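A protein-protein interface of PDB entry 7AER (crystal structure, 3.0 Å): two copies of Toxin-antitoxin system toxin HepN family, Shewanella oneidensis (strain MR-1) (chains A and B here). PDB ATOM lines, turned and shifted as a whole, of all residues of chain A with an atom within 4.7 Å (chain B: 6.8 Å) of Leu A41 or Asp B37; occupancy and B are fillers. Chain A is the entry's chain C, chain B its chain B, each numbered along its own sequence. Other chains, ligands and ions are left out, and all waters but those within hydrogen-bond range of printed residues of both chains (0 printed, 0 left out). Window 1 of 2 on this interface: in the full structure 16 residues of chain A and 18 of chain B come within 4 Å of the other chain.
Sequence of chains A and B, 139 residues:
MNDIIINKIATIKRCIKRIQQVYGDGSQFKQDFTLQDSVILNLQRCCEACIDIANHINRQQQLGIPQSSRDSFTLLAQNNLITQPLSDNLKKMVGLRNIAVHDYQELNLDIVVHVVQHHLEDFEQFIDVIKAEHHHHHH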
ATOM      1  N   ARG A  18       6.573  -3.879 -16.188  1.00  0.00           N
ATOM      2  CA  ARG A  18       5.164  -3.759 -16.536  1.00  0.00           C
ATOM      3  C   ARG A  18       4.470  -2.710 -15.673  1.00  0.00           C
ATOM      4  O   ARG A  18       3.650  -1.931 -16.172  1.00  0.00           O
ATOM      5  CB  ARG A  18       4.486  -5.120 -16.384  1.00  0.00           C
ATOM      6  CG  ARG A  18       3.073  -5.178 -16.904  1.00  0.00           C
ATOM      7  CD  ARG A  18       3.029  -5.626 -18.350  1.00  0.00           C
ATOM      8  NE  ARG A  18       1.764  -5.246 -18.964  1.00  0.00           N
ATOM      9  CZ  ARG A  18       1.554  -4.075 -19.553  1.00  0.00           C
ATOM     10  NH1 ARG A  18       2.529  -3.177 -19.609  1.00  0.00           N
ATOM     11  NH2 ARG A  18       0.373  -3.796 -20.082  1.00  0.00           N
ATOM     12  N   ASP A  37      -5.930  -1.382 -12.387  1.00  0.00           N
ATOM     13  CA  ASP A  37      -6.072  -2.834 -12.368  1.00  0.00           C
ATOM     14  C   ASP A  37      -4.792  -3.524 -12.814  1.00  0.00           C
ATOM     15  O   ASP A  37      -4.393  -4.542 -12.235  1.00  0.00           O
ATOM     16  CB  ASP A  37      -7.243  -3.251 -13.255  1.00  0.00           C
ATOM     17  CG  ASP A  37      -8.578  -2.830 -12.682  1.00  0.00           C
ATOM     18  OD1 ASP A  37      -8.597  -2.334 -11.536  1.00  0.00           O
ATOM     19  OD2 ASP A  37      -9.605  -2.991 -13.374  1.00  0.00           O
ATOM     20  N   SER A  38      -4.136  -2.991 -13.847  1.00  0.00           N
ATOM     21  CA  SER A  38      -2.906  -3.609 -14.331  1.00  0.00           C
ATOM     22  C   SER A  38      -1.779  -3.467 -13.315  1.00  0.00           C
ATOM     23  O   SER A  38      -1.005  -4.409 -13.104  1.00  0.00           O
ATOM     24  CB  SER A  38      -2.503  -2.996 -15.670  1.00  0.00           C
ATOM     25  OG  SER A  38      -1.276  -3.541 -16.123  1.00  0.00           O
ATOM     26  N   VAL A  39      -1.673  -2.303 -12.673  1.00  0.00           N
ATOM     27  CA  VAL A  39      -0.615  -2.091 -11.690  1.00  0.00           C
ATOM     28  C   VAL A  39      -0.840  -2.970 -10.467  1.00  0.00           C
ATOM     29  O   VAL A  39       0.104  -3.564  -9.929  1.00  0.00           O
ATOM     30  CB  VAL A  39      -0.534  -0.600 -11.313  1.00  0.00           C
ATOM     31  CG1 VAL A  39       0.314  -0.405 -10.065  1.00  0.00           C
ATOM     32  CG2 VAL A  39       0.022   0.210 -12.474  1.00  0.00           C
ATOM     33  N   ILE A  40      -2.092  -3.076 -10.013  1.00  0.00           N
ATOM     34  CA  ILE A  40      -2.405  -3.920  -8.864  1.00  0.00           C
ATOM     35  C   ILE A  40      -2.108  -5.382  -9.178  1.00  0.00           C
ATOM     36  O   ILE A  40      -1.580  -6.119  -8.336  1.00  0.00           O
ATOM     37  CB  ILE A  40      -3.870  -3.711  -8.434  1.00  0.00           C
ATOM     38  CG1 ILE A  40      -4.071  -2.295  -7.889  1.00  0.00           C
ATOM     39  CG2 ILE A  40      -4.284  -4.743  -7.397  1.00  0.00           C
ATOM     40  CD1 ILE A  40      -5.525  -1.897  -7.734  1.00  0.00           C
ATOM     41  N   LEU A  41      -2.433  -5.822 -10.396  1.00  0.00           N
ATOM     42  CA  LEU A  41      -2.202  -7.215 -10.767  1.00  0.00           C
ATOM     43  C   LEU A  41      -0.716  -7.553 -10.762  1.00  0.00           C
ATOM     44  O   LEU A  41      -0.299  -8.557 -10.173  1.00  0.00           O
ATOM     45  CB  LEU A  41      -2.806  -7.506 -12.143  1.00  0.00           C
ATOM     46  CG  LEU A  41      -2.577  -8.939 -12.638  1.00  0.00           C
ATOM     47  CD1 LEU A  41      -3.299  -9.934 -11.745  1.00  0.00           C
ATOM     48  CD2 LEU A  41      -2.996  -9.113 -14.089  1.00  0.00           C
ATOM     49  N   ASN A  42       0.100  -6.724 -11.416  1.00  0.00           N
ATOM     50  CA  ASN A  42       1.528  -7.013 -11.500  1.00  0.00           C
ATOM     51  C   ASN A  42       2.231  -6.823 -10.160  1.00  0.00           C
ATOM     52  O   ASN A  42       3.219  -7.513  -9.882  1.00  0.00           O
ATOM     53  CB  ASN A  42       2.174  -6.145 -12.576  1.00  0.00           C
ATOM     54  CG  ASN A  42       1.648  -6.457 -13.961  1.00  0.00           C
ATOM     55  OD1 ASN A  42       1.001  -5.624 -14.594  1.00  0.00           O
ATOM     56  ND2 ASN A  42       1.925  -7.664 -14.440  1.00  0.00           N
ATOM     57  N   LEU A  43       1.752  -5.897  -9.324  1.00  0.00           N
ATOM     58  CA  LEU A  43       2.270  -5.807  -7.963  1.00  0.00           C
ATOM     59  C   LEU A  43       2.009  -7.097  -7.199  1.00  0.00           C
ATOM     60  O   LEU A  43       2.848  -7.547  -6.412  1.00  0.00           O
ATOM     61  CB  LEU A  43       1.646  -4.619  -7.228  1.00  0.00           C
ATOM     62  CG  LEU A  43       2.313  -3.248  -7.352  1.00  0.00           C
ATOM     63  CD1 LEU A  43       1.487  -2.188  -6.642  1.00  0.00           C
ATOM     64  CD2 LEU A  43       3.724  -3.287  -6.783  1.00  0.00           C
ATOM     65  N   GLN A  44       0.846  -7.709  -7.427  1.00  0.00           N
ATOM     66  CA  GLN A  44       0.550  -8.990  -6.798  1.00  0.00           C
ATOM     67  C   GLN A  44       1.450 -10.089  -7.351  1.00  0.00           C
ATOM     68  O   GLN A  44       1.942 -10.934  -6.594  1.00  0.00           O
ATOM     69  CB  GLN A  44      -0.924  -9.330  -6.998  1.00  0.00           C
ATOM     70  CG  GLN A  44      -1.283 -10.773  -6.733  1.00  0.00           C
ATOM     71  CD  GLN A  44      -2.731 -11.063  -7.055  1.00  0.00           C
ATOM     72  OE1 GLN A  44      -3.118 -12.217  -7.247  1.00  0.00           O
ATOM     73  NE2 GLN A  44      -3.543 -10.015  -7.119  1.00  0.00           N
ATOM     74  N   ARG A  45       1.670 -10.094  -8.671  1.00  0.00           N
ATOM     75  CA  ARG A  45       2.551 -11.086  -9.281  1.00  0.00           C
ATOM     76  C   ARG A  45       3.970 -11.001  -8.731  1.00  0.00           C
ATOM     77  O   ARG A  45       4.651 -12.027  -8.616  1.00  0.00           O
ATOM     78  CB  ARG A  45       2.571 -10.918 -10.801  1.00  0.00           C
ATOM     79  CG  ARG A  45       1.295 -11.358 -11.496  1.00  0.00           C
ATOM     80  CD  ARG A  45       1.267 -10.911 -12.949  1.00  0.00           C
ATOM     81  NE  ARG A  45       0.216 -11.584 -13.707  1.00  0.00           N
ATOM     82  CZ  ARG A  45      -0.178 -11.226 -14.925  1.00  0.00           C
ATOM     83  NH1 ARG A  45       0.389 -10.191 -15.531  1.00  0.00           N
ATOM     84  NH2 ARG A  45      -1.141 -11.901 -15.538  1.00  0.00           N
ATOM     85  N   PHE B  29      -7.769  -6.124 -27.704  1.00  0.00           N
ATOM     86  CA  PHE B  29      -7.516  -6.931 -26.514  1.00  0.00           C
ATOM     87  C   PHE B  29      -6.272  -7.797 -26.672  1.00  0.00           C
ATOM     88  O   PHE B  29      -5.340  -7.718 -25.863  1.00  0.00           O
ATOM     89  CB  PHE B  29      -8.733  -7.797 -26.191  1.00  0.00           C
ATOM     90  CG  PHE B  29      -8.558  -8.640 -24.961  1.00  0.00           C
ATOM     91  CD1 PHE B  29      -8.032  -9.921 -25.045  1.00  0.00           C
ATOM     92  CD2 PHE B  29      -8.908  -8.145 -23.717  1.00  0.00           C
ATOM     93  CE1 PHE B  29      -7.865 -10.693 -23.908  1.00  0.00           C
ATOM     94  CE2 PHE B  29      -8.748  -8.912 -22.577  1.00  0.00           C
ATOM     95  CZ  PHE B  29      -8.226 -10.188 -22.672  1.00  0.00           C
ATOM     96  N   ASP B  32      -3.191  -5.632 -26.399  1.00  0.00           N
ATOM     97  CA  ASP B  32      -3.010  -4.702 -25.288  1.00  0.00           C
ATOM     98  C   ASP B  32      -2.871  -5.515 -24.007  1.00  0.00           C
ATOM     99  O   ASP B  32      -3.856  -6.048 -23.487  1.00  0.00           O
ATOM    100  CB  ASP B  32      -4.185  -3.728 -25.203  1.00  0.00           C
ATOM    101  CG  ASP B  32      -3.932  -2.580 -24.243  1.00  0.00           C
ATOM    102  OD1 ASP B  32      -2.916  -2.611 -23.518  1.00  0.00           O
ATOM    103  OD2 ASP B  32      -4.755  -1.642 -24.216  1.00  0.00           O
ATOM    104  N   PHE B  33      -1.637  -5.609 -23.504  1.00  0.00           N
ATOM    105  CA  PHE B  33      -1.396  -6.312 -22.250  1.00  0.00           C
ATOM    106  C   PHE B  33      -2.131  -5.649 -21.092  1.00  0.00           C
ATOM    107  O   PHE B  33      -2.539  -6.330 -20.144  1.00  0.00           O
ATOM    108  CB  PHE B  33       0.105  -6.381 -21.962  1.00  0.00           C
ATOM    109  CG  PHE B  33       0.875  -7.238 -22.930  1.00  0.00           C
ATOM    110  CD1 PHE B  33       0.223  -8.133 -23.763  1.00  0.00           C
ATOM    111  CD2 PHE B  33       2.255  -7.147 -23.004  1.00  0.00           C
ATOM    112  CE1 PHE B  33       0.933  -8.920 -24.653  1.00  0.00           C
ATOM    113  CE2 PHE B  33       2.971  -7.930 -23.892  1.00  0.00           C
ATOM    114  CZ  PHE B  33       2.308  -8.818 -24.718  1.00  0.00           C
ATOM    115  N   THR B  34      -2.295  -4.323 -21.144  1.00  0.00           N
ATOM    116  CA  THR B  34      -2.997  -3.620 -20.075  1.00  0.00           C
ATOM    117  C   THR B  34      -4.458  -4.045 -20.007  1.00  0.00           C
ATOM    118  O   THR B  34      -5.017  -4.208 -18.915  1.00  0.00           O
ATOM    119  CB  THR B  34      -2.878  -2.108 -20.275  1.00  0.00           C
ATOM    120  OG1 THR B  34      -1.493  -1.747 -20.350  1.00  0.00           O
ATOM    121  CG2 THR B  34      -3.519  -1.360 -19.118  1.00  0.00           C
ATOM    122  N   LEU B  35      -5.094  -4.242 -21.165  1.00  0.00           N
ATOM    123  CA  LEU B  35      -6.460  -4.752 -21.169  1.00  0.00           C
ATOM    124  C   LEU B  35      -6.495  -6.186 -20.659  1.00  0.00           C
ATOM    125  O   LEU B  35      -7.440  -6.586 -19.969  1.00  0.00           O
ATOM    126  CB  LEU B  35      -7.054  -4.679 -22.574  1.00  0.00           C
ATOM    127  CG  LEU B  35      -7.308  -3.303 -23.194  1.00  0.00           C
ATOM    128  CD1 LEU B  35      -8.010  -3.463 -24.535  1.00  0.00           C
ATOM    129  CD2 LEU B  35      -8.095  -2.388 -22.269  1.00  0.00           C
ATOM    130  N   GLN B  36      -5.467  -6.972 -20.992  1.00  0.00           N
ATOM    131  CA  GLN B  36      -5.391  -8.341 -20.496  1.00  0.00           C
ATOM    132  C   GLN B  36      -5.236  -8.357 -18.984  1.00  0.00           C
ATOM    133  O   GLN B  36      -5.866  -9.164 -18.293  1.00  0.00           O
ATOM    134  CB  GLN B  36      -4.218  -9.066 -21.154  1.00  0.00           C
ATOM    135  CG  GLN B  36      -4.259  -9.087 -22.671  1.00  0.00           C
ATOM    136  CD  GLN B  36      -2.932  -9.501 -23.277  1.00  0.00           C
ATOM    137  OE1 GLN B  36      -2.072 -10.060 -22.596  1.00  0.00           O
ATOM    138  NE2 GLN B  36      -2.752  -9.208 -24.561  1.00  0.00           N
ATOM    139  N   ASP B  37      -4.393  -7.468 -18.455  1.00  0.00           N
ATOM    140  CA  ASP B  37      -4.174  -7.403 -17.015  1.00  0.00           C
ATOM    141  C   ASP B  37      -5.450  -7.024 -16.275  1.00  0.00           C
ATOM    142  O   ASP B  37      -5.739  -7.565 -15.201  1.00  0.00           O
ATOM    143  CB  ASP B  37      -3.057  -6.409 -16.703  1.00  0.00           C
ATOM    144  CG  ASP B  37      -1.702  -6.890 -17.175  1.00  0.00           C
ATOM    145  OD1 ASP B  37      -1.603  -8.053 -17.622  1.00  0.00           O
ATOM    146  OD2 ASP B  37      -0.734  -6.105 -17.103  1.00  0.00           O
ATOM    147  N   SER B  38      -6.221  -6.087 -16.831  1.00  0.00           N
ATOM    148  CA  SER B  38      -7.435  -5.627 -16.163  1.00  0.00           C
ATOM    149  C   SER B  38      -8.492  -6.722 -16.103  1.00  0.00           C
ATOM    150  O   SER B  38      -9.180  -6.873 -15.087  1.00  0.00           O
ATOM    151  CB  SER B  38      -7.982  -4.389 -16.873  1.00  0.00           C
ATOM    152  OG  SER B  38      -9.198  -3.958 -16.288  1.00  0.00           O
ATOM    153  N   VAL B  39      -8.640  -7.494 -17.181  1.00  0.00           N
ATOM    154  CA  VAL B  39      -9.627  -8.569 -17.197  1.00  0.00           C
ATOM    155  C   VAL B  39      -9.230  -9.677 -16.227  1.00  0.00           C
ATOM    156  O   VAL B  39     -10.076 -10.229 -15.512  1.00  0.00           O
ATOM    157  CB  VAL B  39      -9.812  -9.098 -18.630  1.00  0.00           C
ATOM    158  CG1 VAL B  39     -10.566 -10.421 -18.627  1.00  0.00           C
ATOM    159  CG2 VAL B  39     -10.540  -8.068 -19.482  1.00  0.00           C
ATOM    160  N   ILE B  40      -7.936 -10.007 -16.174  1.00  0.00           N
ATOM    161  CA  ILE B  40      -7.464 -11.063 -15.281  1.00  0.00           C
ATOM    162  C   ILE B  40      -7.721 -10.700 -13.823  1.00  0.00           C
ATOM    163  O   ILE B  40      -8.129 -11.550 -13.021  1.00  0.00           O
ATOM    164  CB  ILE B  40      -5.973 -11.353 -15.542  1.00  0.00           C
ATOM    165  CG1 ILE B  40      -5.785 -11.980 -16.923  1.00  0.00           C
ATOM    166  CG2 ILE B  40      -5.400 -12.256 -14.464  1.00  0.00           C
ATOM    167  CD1 ILE B  40      -4.346 -12.017 -17.385  1.00  0.00           C
ATOM    168  N   LEU B  41      -7.499  -9.436 -13.455  1.00  0.00           N
ATOM    169  CA  LEU B  41      -7.687  -9.028 -12.065  1.00  0.00           C
ATOM    170  C   LEU B  41      -9.142  -9.180 -11.639  1.00  0.00           C
ATOM    171  O   LEU B  41      -9.435  -9.734 -10.572  1.00  0.00           O
ATOM    172  CB  LEU B  41      -7.220  -7.587 -11.866  1.00  0.00           C
ATOM    173  CG  LEU B  41      -7.408  -7.068 -10.438  1.00  0.00           C
ATOM    174  CD1 LEU B  41      -6.529  -7.844  -9.474  1.00  0.00           C
ATOM    175  CD2 LEU B  41      -7.126  -5.581 -10.347  1.00  0.00           C
ATOM    176  N   ASN B  42     -10.072  -8.680 -12.455  1.00  0.00           N
ATOM    177  CA  ASN B  42     -11.482  -8.763 -12.095  1.00  0.00           C
ATOM    178  C   ASN B  42     -11.998 -10.195 -12.164  1.00  0.00           C
ATOM    179  O   ASN B  42     -12.910 -10.559 -11.415  1.00  0.00           O
ATOM    180  CB  ASN B  42     -12.306  -7.847 -12.996  1.00  0.00           C
ATOM    181  CG  ASN B  42     -11.954  -6.386 -12.814  1.00  0.00           C
ATOM    182  OD1 ASN B  42     -11.836  -5.903 -11.689  1.00  0.00           O
ATOM    183  ND2 ASN B  42     -11.785  -5.673 -13.921  1.00  0.00           N
ATOM    184  N   GLN B  44     -10.209 -12.643 -11.160  1.00  0.00           N
ATOM    185  CA  GLN B  44      -9.780 -13.122  -9.850  1.00  0.00           C
ATOM    186  C   GLN B  44     -10.712 -12.623  -8.754  1.00  0.00           C
ATOM    187  O   GLN B  44     -11.069 -13.377  -7.841  1.00  0.00           O
ATOM    188  CB  GLN B  44      -8.345 -12.672  -9.579  1.00  0.00           C
ATOM    189  CG  GLN B  44      -7.916 -12.752  -8.122  1.00  0.00           C
ATOM    190  CD  GLN B  44      -6.529 -12.174  -7.899  1.00  0.00           C
ATOM    191  OE1 GLN B  44      -6.163 -11.818  -6.777  1.00  0.00           O
ATOM    192  NE2 GLN B  44      -5.752 -12.073  -8.971  1.00  0.00           N
ATOM    193  N   ALA B 100      -2.786 -17.566 -14.189  1.00  0.00           N
ATOM    194  CA  ALA B 100      -2.611 -16.175 -14.589  1.00  0.00           C
ATOM    195  C   ALA B 100      -1.896 -15.345 -13.527  1.00  0.00           C
ATOM    196  O   ALA B 100      -1.151 -14.421 -13.873  1.00  0.00           O
ATOM    197  CB  ALA B 100      -3.966 -15.547 -14.915  1.00  0.00           C
ATOM    198  N   VAL B 101      -2.107 -15.644 -12.245  1.00  0.00           N
ATOM    199  CA  VAL B 101      -1.492 -14.875 -11.166  1.00  0.00           C
ATOM    200  C   VAL B 101      -0.011 -15.222 -11.073  1.00  0.00           C
ATOM    201  O   VAL B 101       0.847 -14.417 -11.451  1.00  0.00           O
ATOM    202  CB  VAL B 101      -2.215 -15.114  -9.826  1.00  0.00           C
ATOM    203  CG1 VAL B 101      -1.410 -14.539  -8.672  1.00  0.00           C
ATOM    204  CG2 VAL B 101      -3.599 -14.481  -9.855  1.00  0.00           C
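The side-chain hydroxyl of Thr B34 lies within hydrogen-bond range of the guanidinium group of Arg A18 (2.8 Å).
OD2 of Asp B37 lies within salt-bridge range of NE of Arg A18, at 3.2 Å.
OD2 of Asp B37 sits at hydrogen-bond distance from OG of Ser A38 (2.8 Å).
OD2 of Asp B37 sits close to OD1 of Asn A42 (3.1 Å).
The guanidinium group (NH1) of Arg A45 lies within salt-bridge range of the side-chain carboxylate (OD1) of Asp B37 (3.6 Å).
The side-chain hydroxyl (OG) of Ser B38 sits at hydrogen-bond distance from the side-chain carboxylate (OD2) of Asp A37.
The side-chain amide nitrogen of Asn B42 lies within hydrogen-bond range of the side-chain carboxylate of Asp A37 (3.5 Å).
The side-chain amide oxygen (OE1) of Gln A44 sits close to the side-chain amide oxygen (OE1) of Gln B44, 3.1 Å away.
O of Ala B100 sits at hydrogen-bond distance from NH2 of Arg A45 (3.0 Å).
The side-chain carboxylate (OD1) of Asp B32 sits at hydrogen-bond distance from the backbone NH (N) of Thr B34.
ND2 of Asn B42 sits at hydrogen-bond distance from O of Ser B38 (3.1 Å).
The backbone carbonyl oxygen (O) of Ser A38 sits close to the side-chain amide oxygen (OD1) of Asn A42 (2.8 Å).
NH1 of Arg A45 sits close to ND2 of Asn A42 (3.2 Å).
Among the printed residues, pairs that only touch across the chains: Arg A18 with Phe B33 (3.2 Å), Asp A37 with Leu B41 (3.5 Å), Ser A38 with Thr B34 (3.9 Å), Leu A41 with Asp B37 (3.3 Å), Leu A41 with Ile B40 (3.97 Å), Gln A44 with Val B101 (3.2 Å), Arg A45 with Ile B40 (3.7 Å) and Arg A45 with Val B101 (3.1 Å).
Of chain B, only Asp B37 (3.3 Å) and Ile B40 (3.97 Å) come within 4 Å of Leu A41.
Of the printed residues of chain A, Asp B37 touches Arg A18 (3.2 Å), Ser A38 (2.8 Å), Leu A41 (3.3 Å), Asn A42 (3.1 Å) and Arg A45 (3.6 Å).
Of the printed residues of chain A, Thr B34 touches Arg A18 (2.8 Å) and Ser A38 (3.9 Å).
Of the printed residues of chain B, Asn A42 touches Asp B37.
Leu A43 touches none of the printed residues of chain B.
The nearest residue of chain B that does not touch Leu A41 is Gln B44 (4.3 Å).
The nearest residue of chain A that does not touch Asp B37 is Asp A37 (4.4 Å).
The nearest printed residue of chain A that does not touch Gln B44 is Leu A41 (4.3 Å).
Hydrophobic or aromatic side chains of chain B that line the printed part of chain A: Phe B33, Ile B40, Leu B41 and Val B101.
Hydrophobic or aromatic side chains of chain A that line the printed part of chain B: Leu A41.
Along chain A the printed residues that touch a printed residue of chain B span positions 18 to 45.
Asp A37 touches Ser B38, and with the chains exchanged Ser A38 touches Asp B37.
Asp A37 touches Leu B41, and with the chains exchanged Leu A41 touches Asp B37.
Leu A41 touches Ile B40, but with the chains exchanged Ile A40 does not touch Leu B41 (4.2 Å).
Gln A44 touches its own counterpart, Gln B44.
Of the 17 pairs that touch across the chains among the printed residues, 7 have their exchanged pair printed and touching as well.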
